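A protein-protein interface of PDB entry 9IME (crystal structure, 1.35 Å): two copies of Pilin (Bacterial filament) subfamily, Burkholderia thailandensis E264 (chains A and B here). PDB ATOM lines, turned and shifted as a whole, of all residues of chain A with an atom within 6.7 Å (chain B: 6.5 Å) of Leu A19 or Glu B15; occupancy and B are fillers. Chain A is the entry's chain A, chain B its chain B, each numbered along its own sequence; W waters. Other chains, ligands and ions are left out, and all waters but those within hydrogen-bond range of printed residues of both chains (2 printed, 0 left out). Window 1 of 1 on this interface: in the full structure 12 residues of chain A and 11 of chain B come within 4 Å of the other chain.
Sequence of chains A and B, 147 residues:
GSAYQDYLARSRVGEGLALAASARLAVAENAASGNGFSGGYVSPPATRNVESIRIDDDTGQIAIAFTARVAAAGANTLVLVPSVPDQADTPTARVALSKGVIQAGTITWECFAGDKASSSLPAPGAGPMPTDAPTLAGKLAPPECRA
OE2 of Glu A15 is in salt-bridge range of NH1 of Arg B48.
The guanidinium group (NE) of Arg B48 lies close to the guanidinium group (NE) of Arg A48, 3.4 Å away.
The guanidinium group (NH1) of Arg A48 sits close to the guanidinium group (NH2) of Arg B69.
Of the printed residues of chain B, Glu A15 touches Thr B47 (3.8 Å) and Arg B48 (3.5 Å).
Of the printed residues of chain B, Leu A19 touches Glu B15 (3.6 Å) and Leu B19 (3.6 Å).
Of the printed residues of chain B, Ala A21 touches Ala B18 and Ala B21.
Of the printed residues of chain B, Pro A44 touches Ala B18 (3.7 Å).
Printed residues of chain B within 4 Å of Thr A47: Glu B15 and Arg B48.
Arg B10 touches none of the printed residues of chain A.
Of the printed residues of chain A, Ser B11 touches Pro A45.
Printed residues of chain A within 4 Å of Glu B15: Leu A19 and Thr A47.
The nearest printed residue of chain B that does not touch Leu A19 is Ala B18 (4.02 Å).
The nearest printed residue of chain A that does not touch Glu B15 is Pro A45 (4.3 Å).
The nearest printed residue of chain B that does not touch Ser A22 is Leu B19 (5.6 Å).
Water W2 lies within hydrogen-bond range of the side-chain carboxylate (OE1) of Glu A15 and the guanidinium group (NH1) of Arg B48.
Water W1 lies within hydrogen-bond range of the backbone carbonyl oxygen (O) of Ala A18 (2.8 Å) and the backbone carbonyl oxygen (O) of Leu B19 (2.9 Å).
Glu A15 touches Thr B47, and with the chains exchanged Thr A47 touches Glu B15.
Ala A18 touches Leu B19, but with the chains exchanged Leu A19 does not touch Ala B18 (4.02 Å).
Thr A47 touches Arg B48, but with the chains exchanged Arg A48 does not touch Thr B47 (9.1 Å).
Arg A48 touches its own counterpart, Arg B48.
12 positions are printed for both chains.
CB of Thr B47 touches OE1 of Glu A15, 3.8 Å away.
CD2 of Leu B19 touches C of Ala A18, at 3.5 Å.
Leu A19 touches Glu B15 (CD2 to O, 3.6 Å).
Leu A19 touches Leu B19.
N of Ser A22 touches O of Ala B18, at 3.6 Å.
N of Ser A22 touches CB of Ala B21, at 3.6 Å.
CB of Pro A44 touches CB of Ala B18 (3.7 Å).
Ser B11 touches Pro A45 (OG to CB, 3.2 Å).
CD of Glu B15 touches CG2 of Thr A47 (3.6 Å).
NH2 of Arg B48 touches CB of Thr A47, at 3.4 Å.
Of the 20 printed residues of chain A, 9 touch a printed residue of chain B.
Printed residues of chain B that touch a printed residue of chain A: Ser B11, Glu B15, Ala B18, Leu B19, Ala B21, Thr B47, Arg B48 and Arg B69.
Among the printed residues, Asp or Glu carboxylates within 4 Å of a Lys or Arg side-chain nitrogen of the other chain: Glu A15 with Arg B48 (3.5 Å).
O of Leu A19 sits at hydrogen-bond distance from OG of Ser A22 (2.8 Å).
The side-chain hydroxyl (OH) of Tyr A41 is in hydrogen-bond range of the side-chain hydroxyl (OG) of Ser A22 (3.0 Å).
OG1 of Thr A47 is in hydrogen-bond range of N of Val A50, at 2.9 Å.
The guanidinium group (NH1) of Arg B12 is in hydrogen-bond range of the backbone carbonyl oxygen (O) of Arg B69 (3.1 Å).
The side-chain hydroxyl of Thr B47 sits close to the backbone NH of Asn B49 (3.1 Å).
The side-chain amide oxygen of Asn B49 lies within hydrogen-bond range of the guanidinium group of Arg B69, at 2.4 Å.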
ATOM      1  N   GLY A  14      -0.810  24.210   5.668  1.00  0.00           N
ATOM      2  CA  GLY A  14      -0.702  23.261   6.765  1.00  0.00           C
ATOM      3  C   GLY A  14      -0.916  23.907   8.120  1.00  0.00           C
ATOM      4  O   GLY A  14      -1.535  23.317   9.012  1.00  0.00           O
ATOM      5  N   GLU A  15      -0.424  25.135   8.289  1.00  0.00           N
ATOM      6  CA  GLU A  15      -0.650  25.852   9.536  1.00  0.00           C
ATOM      7  C   GLU A  15      -2.129  26.154   9.734  1.00  0.00           C
ATOM      8  O   GLU A  15      -2.649  26.024  10.847  1.00  0.00           O
ATOM      9  CB  GLU A  15       0.181  27.134   9.562  1.00  0.00           C
ATOM     10  CG  GLU A  15       1.680  26.881   9.658  1.00  0.00           C
ATOM     11  CD  GLU A  15       2.515  28.155   9.661  1.00  0.00           C
ATOM     12  OE1 GLU A  15       3.611  28.126  10.255  1.00  0.00           O
ATOM     13  OE2 GLU A  15       2.087  29.177   9.073  1.00  0.00           O
ATOM     14  N   GLY A  16      -2.828  26.539   8.667  1.00  0.00           N
ATOM     15  CA  GLY A  16      -4.257  26.772   8.786  1.00  0.00           C
ATOM     16  C   GLY A  16      -5.018  25.518   9.169  1.00  0.00           C
ATOM     17  O   GLY A  16      -5.922  25.557  10.008  1.00  0.00           O
ATOM     18  N   LEU A  17      -4.663  24.386   8.562  1.00  0.00           N
ATOM     19  CA  LEU A  17      -5.304  23.130   8.924  1.00  0.00           C
ATOM     20  C   LEU A  17      -5.075  22.812  10.392  1.00  0.00           C
ATOM     21  O   LEU A  17      -5.977  22.327  11.083  1.00  0.00           O
ATOM     22  CB  LEU A  17      -4.747  22.010   8.053  1.00  0.00           C
ATOM     23  CG  LEU A  17      -5.334  21.985   6.655  1.00  0.00           C
ATOM     24  CD1 LEU A  17      -4.436  21.164   5.748  1.00  0.00           C
ATOM     25  CD2 LEU A  17      -6.757  21.434   6.709  1.00  0.00           C
ATOM     26  N   ALA A  18      -3.875  23.089  10.887  1.00  0.00           N
ATOM     27  CA  ALA A  18      -3.600  22.822  12.291  1.00  0.00           C
ATOM     28  C   ALA A  18      -4.392  23.763  13.194  1.00  0.00           C
ATOM     29  O   ALA A  18      -4.914  23.340  14.232  1.00  0.00           O
ATOM     30  CB  ALA A  18      -2.096  22.917  12.549  1.00  0.00           C
ATOM     31  N   LEU A  19      -4.501  25.042  12.820  1.00  0.00           N
ATOM     32  CA  LEU A  19      -5.313  25.965  13.610  1.00  0.00           C
ATOM     33  C   LEU A  19      -6.778  25.557  13.643  1.00  0.00           C
ATOM     34  O   LEU A  19      -7.486  25.855  14.613  1.00  0.00           O
ATOM     35  CB  LEU A  19      -5.180  27.390  13.078  1.00  0.00           C
ATOM     36  CG  LEU A  19      -3.864  28.107  13.405  1.00  0.00           C
ATOM     37  CD1 LEU A  19      -3.667  29.327  12.525  1.00  0.00           C
ATOM     38  CD2 LEU A  19      -3.825  28.487  14.886  1.00  0.00           C
ATOM     39  N   ALA A  20      -7.244  24.872  12.605  1.00  0.00           N
ATOM     40  CA  ALA A  20      -8.619  24.399  12.550  1.00  0.00           C
ATOM     41  C   ALA A  20      -8.894  23.240  13.501  1.00  0.00           C
ATOM     42  O   ALA A  20     -10.047  22.816  13.612  1.00  0.00           O
ATOM     43  CB  ALA A  20      -8.991  24.037  11.111  1.00  0.00           C
ATOM     44  N   ALA A  21      -7.876  22.724  14.202  1.00  0.00           N
ATOM     45  CA  ALA A  21      -8.141  21.741  15.246  1.00  0.00           C
ATOM     46  C   ALA A  21      -9.132  22.279  16.260  1.00  0.00           C
ATOM     47  O   ALA A  21      -9.944  21.519  16.792  1.00  0.00           O
ATOM     48  CB  ALA A  21      -6.844  21.349  15.947  1.00  0.00           C
ATOM     49  N   SER A  22      -9.082  23.590  16.526  1.00  0.00           N
ATOM     50  CA  SER A  22     -10.032  24.222  17.432  1.00  0.00           C
ATOM     51  C   SER A  22     -11.459  23.990  16.972  1.00  0.00           C
ATOM     52  O   SER A  22     -12.351  23.721  17.785  1.00  0.00           O
ATOM     53  CB  SER A  22      -9.752  25.733  17.498  1.00  0.00           C
ATOM     54  OG  SER A  22      -9.766  26.320  16.191  1.00  0.00           O
ATOM     55  N   ALA A  23     -11.695  24.107  15.666  1.00  0.00           N
ATOM     56  CA  ALA A  23     -13.027  23.883  15.129  1.00  0.00           C
ATOM     57  C   ALA A  23     -13.388  22.403  15.139  1.00  0.00           C
ATOM     58  O   ALA A  23     -14.544  22.054  15.383  1.00  0.00           O
ATOM     59  CB  ALA A  23     -13.106  24.457  13.720  1.00  0.00           C
ATOM     60  N   ARG A  24     -12.424  21.514  14.875  1.00  0.00           N
ATOM     61  CA  ARG A  24     -12.729  20.085  14.931  1.00  0.00           C
ATOM     62  C   ARG A  24     -13.148  19.676  16.338  1.00  0.00           C
ATOM     63  O   ARG A  24     -14.062  18.858  16.510  1.00  0.00           O
ATOM     64  CB  ARG A  24     -11.530  19.267  14.458  1.00  0.00           C
ATOM     65  CG  ARG A  24     -11.231  19.438  12.962  1.00  0.00           C
ATOM     66  CD  ARG A  24     -10.138  18.475  12.420  1.00  0.00           C
ATOM     67  NE  ARG A  24      -8.805  18.741  12.958  1.00  0.00           N
ATOM     68  CZ  ARG A  24      -7.883  19.534  12.412  1.00  0.00           C
ATOM     69  NH1 ARG A  24      -8.120  20.234  11.308  1.00  0.00           N
ATOM     70  NH2 ARG A  24      -6.688  19.627  12.986  1.00  0.00           N
ATOM     71  N   TYR A  41     -18.418  28.217  19.292  1.00  0.00           N
ATOM     72  CA  TYR A  41     -17.074  28.211  18.738  1.00  0.00           C
ATOM     73  C   TYR A  41     -16.592  29.631  18.505  1.00  0.00           C
ATOM     74  O   TYR A  41     -17.274  30.427  17.852  1.00  0.00           O
ATOM     75  CB  TYR A  41     -17.039  27.451  17.414  1.00  0.00           C
ATOM     76  CG  TYR A  41     -15.703  27.546  16.724  1.00  0.00           C
ATOM     77  CD1 TYR A  41     -14.555  27.023  17.309  1.00  0.00           C
ATOM     78  CD2 TYR A  41     -15.585  28.163  15.483  1.00  0.00           C
ATOM     79  CE1 TYR A  41     -13.324  27.111  16.678  1.00  0.00           C
ATOM     80  CE2 TYR A  41     -14.362  28.243  14.845  1.00  0.00           C
ATOM     81  CZ  TYR A  41     -13.237  27.710  15.448  1.00  0.00           C
ATOM     82  OH  TYR A  41     -12.015  27.800  14.809  1.00  0.00           O
ATOM     83  N   PRO A  44      -9.703  31.231  16.438  1.00  0.00           N
ATOM     84  CA  PRO A  44      -8.505  31.927  16.901  1.00  0.00           C
ATOM     85  C   PRO A  44      -8.325  33.227  16.144  1.00  0.00           C
ATOM     86  O   PRO A  44      -9.002  33.465  15.132  1.00  0.00           O
ATOM     87  CB  PRO A  44      -7.379  30.937  16.573  1.00  0.00           C
ATOM     88  CG  PRO A  44      -7.917  30.092  15.480  1.00  0.00           C
ATOM     89  CD  PRO A  44      -9.378  29.966  15.751  1.00  0.00           C
ATOM     90  N   PRO A  45      -7.442  34.107  16.609  1.00  0.00           N
ATOM     91  CA  PRO A  45      -7.217  35.362  15.889  1.00  0.00           C
ATOM     92  C   PRO A  45      -6.812  35.106  14.448  1.00  0.00           C
ATOM     93  O   PRO A  45      -6.143  34.122  14.129  1.00  0.00           O
ATOM     94  CB  PRO A  45      -6.069  36.015  16.664  1.00  0.00           C
ATOM     95  CG  PRO A  45      -6.166  35.432  18.036  1.00  0.00           C
ATOM     96  CD  PRO A  45      -6.646  34.028  17.848  1.00  0.00           C
ATOM     97  N   ALA A  46      -7.229  36.010  13.571  1.00  0.00           N
ATOM     98  CA  ALA A  46      -6.713  35.982  12.216  1.00  0.00           C
ATOM     99  C   ALA A  46      -5.197  36.146  12.249  1.00  0.00           C
ATOM    100  O   ALA A  46      -4.639  36.822  13.116  1.00  0.00           O
ATOM    101  CB  ALA A  46      -7.355  37.098  11.389  1.00  0.00           C
ATOM    102  N   THR A  47      -4.523  35.493  11.314  1.00  0.00           N
ATOM    103  CA  THR A  47      -3.077  35.579  11.200  1.00  0.00           C
ATOM    104  C   THR A  47      -2.730  36.165   9.838  1.00  0.00           C
ATOM    105  O   THR A  47      -3.606  36.426   9.008  1.00  0.00           O
ATOM    106  CB  THR A  47      -2.429  34.202  11.379  1.00  0.00           C
ATOM    107  OG1 THR A  47      -2.593  33.448  10.175  1.00  0.00           O
ATOM    108  CG2 THR A  47      -3.067  33.439  12.532  1.00  0.00           C
ATOM    109  N   ARG A  48      -1.432  36.353   9.595  1.00  0.00           N
ATOM    110  CA  ARG A  48      -1.020  36.818   8.277  1.00  0.00           C
ATOM    111  C   ARG A  48      -1.439  35.847   7.183  1.00  0.00           C
ATOM    112  O   ARG A  48      -1.550  36.250   6.020  1.00  0.00           O
ATOM    113  CB  ARG A  48       0.497  36.992   8.205  1.00  0.00           C
ATOM    114  CG  ARG A  48       1.265  35.728   8.539  1.00  0.00           C
ATOM    115  CD  ARG A  48       2.741  36.001   8.757  1.00  0.00           C
ATOM    116  NE  ARG A  48       3.015  36.668  10.020  1.00  0.00           N
ATOM    117  CZ  ARG A  48       4.228  37.017  10.423  1.00  0.00           C
ATOM    118  NH1 ARG A  48       4.418  37.657  11.564  1.00  0.00           N
ATOM    119  NH2 ARG A  48       5.278  36.708   9.664  1.00  0.00           N
ATOM    120  N   VAL A  50      -4.103  33.131   7.683  1.00  0.00           N
ATOM    121  CA  VAL A  50      -5.450  32.588   7.828  1.00  0.00           C
ATOM    122  C   VAL A  50      -6.411  33.739   8.097  1.00  0.00           C
ATOM    123  O   VAL A  50      -6.326  34.403   9.138  1.00  0.00           O
ATOM    124  CB  VAL A  50      -5.509  31.537   8.944  1.00  0.00           C
ATOM    125  CG1 VAL A  50      -6.923  30.969   9.071  1.00  0.00           C
ATOM    126  CG2 VAL A  50      -4.516  30.441   8.651  1.00  0.00           C
ATOM    127  N   ILE A  53     -11.718  30.900  10.087  1.00  0.00           N
ATOM    128  CA  ILE A  53     -12.109  29.504  10.210  1.00  0.00           C
ATOM    129  C   ILE A  53     -13.547  29.507  10.700  1.00  0.00           C
ATOM    130  O   ILE A  53     -13.844  30.127  11.728  1.00  0.00           O
ATOM    131  CB  ILE A  53     -11.221  28.750  11.217  1.00  0.00           C
ATOM    132  CG1 ILE A  53      -9.750  28.862  10.793  1.00  0.00           C
ATOM    133  CG2 ILE A  53     -11.687  27.286  11.340  1.00  0.00           C
ATOM    134  CD1 ILE A  53      -8.772  28.320  11.820  1.00  0.00           C
ATOM    135  N   ILE A  64     -11.832  26.950   5.872  1.00  0.00           N
ATOM    136  CA  ILE A  64     -10.659  27.752   6.209  1.00  0.00           C
ATOM    137  C   ILE A  64     -10.389  28.658   5.019  1.00  0.00           C
ATOM    138  O   ILE A  64     -10.179  28.171   3.898  1.00  0.00           O
ATOM    139  CB  ILE A  64      -9.422  26.876   6.468  1.00  0.00           C
ATOM    140  CG1 ILE A  64      -9.719  25.781   7.498  1.00  0.00           C
ATOM    141  CG2 ILE A  64      -8.228  27.748   6.900  1.00  0.00           C
ATOM    142  CD1 ILE A  64      -8.633  24.719   7.563  1.00  0.00           C
ATOM    143  N   ARG B  10      -0.709  37.939  23.698  1.00  0.00           N
ATOM    144  CA  ARG B  10      -1.920  37.196  24.031  1.00  0.00           C
ATOM    145  C   ARG B  10      -2.590  36.644  22.779  1.00  0.00           C
ATOM    146  O   ARG B  10      -3.136  35.536  22.792  1.00  0.00           O
ATOM    147  CB  ARG B  10      -2.890  38.092  24.795  1.00  0.00           C
ATOM    148  CG  ARG B  10      -2.490  38.299  26.246  1.00  0.00           C
ATOM    149  CD  ARG B  10      -3.635  38.877  27.045  1.00  0.00           C
ATOM    150  NE  ARG B  10      -4.000  40.204  26.574  1.00  0.00           N
ATOM    151  CZ  ARG B  10      -3.415  41.329  26.961  1.00  0.00           C
ATOM    152  NH1 ARG B  10      -2.409  41.324  27.823  1.00  0.00           N
ATOM    153  NH2 ARG B  10      -3.857  42.489  26.479  1.00  0.00           N
ATOM    154  N   SER B  11      -2.558  37.407  21.687  1.00  0.00           N
ATOM    155  CA  SER B  11      -3.153  36.935  20.445  1.00  0.00           C
ATOM    156  C   SER B  11      -2.417  35.701  19.949  1.00  0.00           C
ATOM    157  O   SER B  11      -3.037  34.728  19.498  1.00  0.00           O
ATOM    158  CB  SER B  11      -3.078  38.041  19.395  1.00  0.00           C
ATOM    159  OG  SER B  11      -3.787  37.673  18.236  1.00  0.00           O
ATOM    160  N   ARG B  12      -1.088  35.724  20.040  1.00  0.00           N
ATOM    161  CA  ARG B  12      -0.291  34.601  19.576  1.00  0.00           C
ATOM    162  C   ARG B  12      -0.452  33.397  20.490  1.00  0.00           C
ATOM    163  O   ARG B  12      -0.431  32.254  20.017  1.00  0.00           O
ATOM    164  CB  ARG B  12       1.173  35.033  19.447  1.00  0.00           C
ATOM    165  CG  ARG B  12       1.379  36.079  18.358  1.00  0.00           C
ATOM    166  CD  ARG B  12       2.589  36.969  18.617  1.00  0.00           C
ATOM    167  NE  ARG B  12       2.605  38.113  17.707  1.00  0.00           N
ATOM    168  CZ  ARG B  12       3.566  39.026  17.671  1.00  0.00           C
ATOM    169  NH1 ARG B  12       4.608  38.962  18.480  1.00  0.00           N
ATOM    170  NH2 ARG B  12       3.469  40.036  16.810  1.00  0.00           N
ATOM    171  N   VAL B  13      -0.645  33.634  21.790  1.00  0.00           N
ATOM    172  CA  VAL B  13      -0.943  32.546  22.717  1.00  0.00           C
ATOM    173  C   VAL B  13      -2.284  31.914  22.374  1.00  0.00           C
ATOM    174  O   VAL B  13      -2.455  30.693  22.474  1.00  0.00           O
ATOM    175  CB  VAL B  13      -0.878  33.053  24.171  1.00  0.00           C
ATOM    176  CG1 VAL B  13      -1.512  32.039  25.120  1.00  0.00           C
ATOM    177  CG2 VAL B  13       0.570  33.317  24.576  1.00  0.00           C
ATOM    178  N   GLY B  14      -3.245  32.732  21.935  1.00  0.00           N
ATOM    179  CA  GLY B  14      -4.518  32.195  21.482  1.00  0.00           C
ATOM    180  C   GLY B  14      -4.365  31.260  20.299  1.00  0.00           C
ATOM    181  O   GLY B  14      -5.077  30.256  20.195  1.00  0.00           O
ATOM    182  N   GLU B  15      -3.441  31.574  19.391  1.00  0.00           N
ATOM    183  CA  GLU B  15      -3.140  30.648  18.303  1.00  0.00           C
ATOM    184  C   GLU B  15      -2.645  29.313  18.847  1.00  0.00           C
ATOM    185  O   GLU B  15      -3.075  28.248  18.395  1.00  0.00           O
ATOM    186  CB  GLU B  15      -2.102  31.261  17.364  1.00  0.00           C
ATOM    187  CG  GLU B  15      -2.577  32.494  16.616  1.00  0.00           C
ATOM    188  CD  GLU B  15      -1.473  33.111  15.777  1.00  0.00           C
ATOM    189  OE1 GLU B  15      -1.413  34.357  15.687  1.00  0.00           O
ATOM    190  OE2 GLU B  15      -0.664  32.346  15.208  1.00  0.00           O
ATOM    191  N   GLY B  16      -1.734  29.351  19.821  1.00  0.00           N
ATOM    192  CA  GLY B  16      -1.234  28.108  20.381  1.00  0.00           C
ATOM    193  C   GLY B  16      -2.307  27.303  21.086  1.00  0.00           C
ATOM    194  O   GLY B  16      -2.325  26.071  21.005  1.00  0.00           O
ATOM    195  N   LEU B  17      -3.217  27.979  21.785  1.00  0.00           N
ATOM    196  CA  LEU B  17      -4.315  27.260  22.422  1.00  0.00           C
ATOM    197  C   LEU B  17      -5.214  26.598  21.383  1.00  0.00           C
ATOM    198  O   LEU B  17      -5.721  25.490  21.600  1.00  0.00           O
ATOM    199  CB  LEU B  17      -5.106  28.189  23.341  1.00  0.00           C
ATOM    200  CG  LEU B  17      -4.360  28.588  24.615  1.00  0.00           C
ATOM    201  CD1 LEU B  17      -5.012  29.796  25.263  1.00  0.00           C
ATOM    202  CD2 LEU B  17      -4.316  27.417  25.591  1.00  0.00           C
ATOM    203  N   ALA B  18      -5.420  27.261  20.242  1.00  0.00           N
ATOM    204  CA  ALA B  18      -6.182  26.643  19.163  1.00  0.00           C
ATOM    205  C   ALA B  18      -5.461  25.420  18.616  1.00  0.00           C
ATOM    206  O   ALA B  18      -6.083  24.373  18.403  1.00  0.00           O
ATOM    207  CB  ALA B  18      -6.425  27.657  18.050  1.00  0.00           C
ATOM    208  N   LEU B  19      -4.150  25.531  18.385  1.00  0.00           N
ATOM    209  CA  LEU B  19      -3.377  24.377  17.931  1.00  0.00           C
ATOM    210  C   LEU B  19      -3.485  23.219  18.917  1.00  0.00           C
ATOM    211  O   LEU B  19      -3.574  22.055  18.511  1.00  0.00           O
ATOM    212  CB  LEU B  19      -1.913  24.765  17.729  1.00  0.00           C
ATOM    213  CG  LEU B  19      -1.590  25.761  16.620  1.00  0.00           C
ATOM    214  CD1 LEU B  19      -0.116  26.146  16.667  1.00  0.00           C
ATOM    215  CD2 LEU B  19      -1.937  25.186  15.276  1.00  0.00           C
ATOM    216  N   ALA B  20      -3.510  23.526  20.216  1.00  0.00           N
ATOM    217  CA  ALA B  20      -3.547  22.517  21.266  1.00  0.00           C
ATOM    218  C   ALA B  20      -4.867  21.769  21.312  1.00  0.00           C
ATOM    219  O   ALA B  20      -4.956  20.754  22.007  1.00  0.00           O
ATOM    220  CB  ALA B  20      -3.264  23.155  22.624  1.00  0.00           C
ATOM    221  N   ALA B  21      -5.880  22.216  20.569  1.00  0.00           N
ATOM    222  CA  ALA B  21      -7.113  21.446  20.509  1.00  0.00           C
ATOM    223  C   ALA B  21      -6.877  20.050  19.954  1.00  0.00           C
ATOM    224  O   ALA B  21      -7.598  19.112  20.305  1.00  0.00           O
ATOM    225  CB  ALA B  21      -8.134  22.178  19.651  1.00  0.00           C
ATOM    226  N   THR B  47       5.407  26.614  14.514  1.00  0.00           N
ATOM    227  CA  THR B  47       5.094  27.861  13.835  1.00  0.00           C
ATOM    228  C   THR B  47       6.016  28.964  14.352  1.00  0.00           C
ATOM    229  O   THR B  47       6.816  28.768  15.272  1.00  0.00           O
ATOM    230  CB  THR B  47       3.616  28.235  14.014  1.00  0.00           C
ATOM    231  OG1 THR B  47       3.409  28.784  15.322  1.00  0.00           O
ATOM    232  CG2 THR B  47       2.719  27.010  13.833  1.00  0.00           C
ATOM    233  N   ARG B  48       5.899  30.144  13.746  1.00  0.00           N
ATOM    234  CA  ARG B  48       6.641  31.295  14.243  1.00  0.00           C
ATOM    235  C   ARG B  48       6.287  31.633  15.689  1.00  0.00           C
ATOM    236  O   ARG B  48       7.052  32.340  16.348  1.00  0.00           O
ATOM    237  CB  ARG B  48       6.389  32.508  13.353  1.00  0.00           C
ATOM    238  CG  ARG B  48       4.954  32.983  13.389  1.00  0.00           C
ATOM    239  CD  ARG B  48       4.561  33.636  12.074  1.00  0.00           C
ATOM    240  NE  ARG B  48       3.144  33.975  12.045  1.00  0.00           N
ATOM    241  CZ  ARG B  48       2.197  33.180  11.566  1.00  0.00           C
ATOM    242  NH1 ARG B  48       2.488  32.001  11.041  1.00  0.00           N
ATOM    243  NH2 ARG B  48       0.929  33.580  11.611  1.00  0.00           N
ATOM    244  N   ASN B  49       5.156  31.133  16.202  1.00  0.00           N
ATOM    245  CA  ASN B  49       4.708  31.427  17.560  1.00  0.00           C
ATOM    246  C   ASN B  49       4.763  30.254  18.526  1.00  0.00           C
ATOM    247  O   ASN B  49       4.848  30.480  19.742  1.00  0.00           O
ATOM    248  CB  ASN B  49       3.271  31.968  17.536  1.00  0.00           C
ATOM    249  CG  ASN B  49       3.167  33.283  16.802  1.00  0.00           C
ATOM    250  OD1 ASN B  49       4.100  34.088  16.831  1.00  0.00           O
ATOM    251  ND2 ASN B  49       2.066  33.484  16.088  1.00  0.00           N
ATOM    252  N   VAL B  50       4.717  29.019  18.034  1.00  0.00           N
ATOM    253  CA  VAL B  50       4.575  27.843  18.884  1.00  0.00           C
ATOM    254  C   VAL B  50       5.707  26.882  18.574  1.00  0.00           C
ATOM    255  O   VAL B  50       5.869  26.460  17.421  1.00  0.00           O
ATOM    256  CB  VAL B  50       3.218  27.153  18.671  1.00  0.00           C
ATOM    257  CG1 VAL B  50       3.095  25.937  19.571  1.00  0.00           C
ATOM    258  CG2 VAL B  50       2.091  28.140  18.931  1.00  0.00           C
ATOM    259  N   ILE B  53       3.876  21.240  21.260  1.00  0.00           N
ATOM    260  CA  ILE B  53       2.722  20.931  22.096  1.00  0.00           C
ATOM    261  C   ILE B  53       2.815  19.447  22.410  1.00  0.00           C
ATOM    262  O   ILE B  53       2.751  18.616  21.497  1.00  0.00           O
ATOM    263  CB  ILE B  53       1.394  21.250  21.393  1.00  0.00           C
ATOM    264  CG1 ILE B  53       1.331  22.739  21.043  1.00  0.00           C
ATOM    265  CG2 ILE B  53       0.226  20.839  22.279  1.00  0.00           C
ATOM    266  CD1 ILE B  53       0.137  23.147  20.239  1.00  0.00           C
ATOM    267  N   PHE B  66       5.934  28.274  23.731  1.00  0.00           N
ATOM    268  CA  PHE B  66       5.890  29.363  22.763  1.00  0.00           C
ATOM    269  C   PHE B  66       7.297  29.825  22.389  1.00  0.00           C
ATOM    270  O   PHE B  66       8.255  29.643  23.145  1.00  0.00           O
ATOM    271  CB  PHE B  66       5.053  30.528  23.318  1.00  0.00           C
ATOM    272  CG  PHE B  66       3.603  30.188  23.466  1.00  0.00           C
ATOM    273  CD1 PHE B  66       3.094  29.774  24.687  1.00  0.00           C
ATOM    274  CD2 PHE B  66       2.750  30.235  22.371  1.00  0.00           C
ATOM    275  CE1 PHE B  66       1.759  29.435  24.823  1.00  0.00           C
ATOM    276  CE2 PHE B  66       1.414  29.889  22.493  1.00  0.00           C
ATOM    277  CZ  PHE B  66       0.911  29.485  23.720  1.00  0.00           C
ATOM    278  N   ARG B  69       8.966  35.056  19.958  1.00  0.00           N
ATOM    279  CA  ARG B  69       7.980  36.025  19.498  1.00  0.00           C
ATOM    280  C   ARG B  69       6.895  36.278  20.538  1.00  0.00           C
ATOM    281  O   ARG B  69       6.219  37.313  20.479  1.00  0.00           O
ATOM    282  CB  ARG B  69       7.344  35.514  18.205  1.00  0.00           C
ATOM    283  CG  ARG B  69       7.134  36.580  17.159  1.00  0.00           C
ATOM    284  CD  ARG B  69       6.567  36.000  15.875  1.00  0.00           C
ATOM    285  NE  ARG B  69       5.830  37.019  15.137  1.00  0.00           N
ATOM    286  CZ  ARG B  69       4.511  37.040  14.999  1.00  0.00           C
ATOM    287  NH1 ARG B  69       3.747  36.077  15.490  1.00  0.00           N
ATOM    288  NH2 ARG B  69       3.944  38.054  14.355  1.00  0.00           N
HETATM  289  O   HOH W   1      -3.324  21.511  15.676  1.00  0.00           O
HETATM  290  O   HOH W   2       4.421  30.164  11.267  1.00  0.00           O
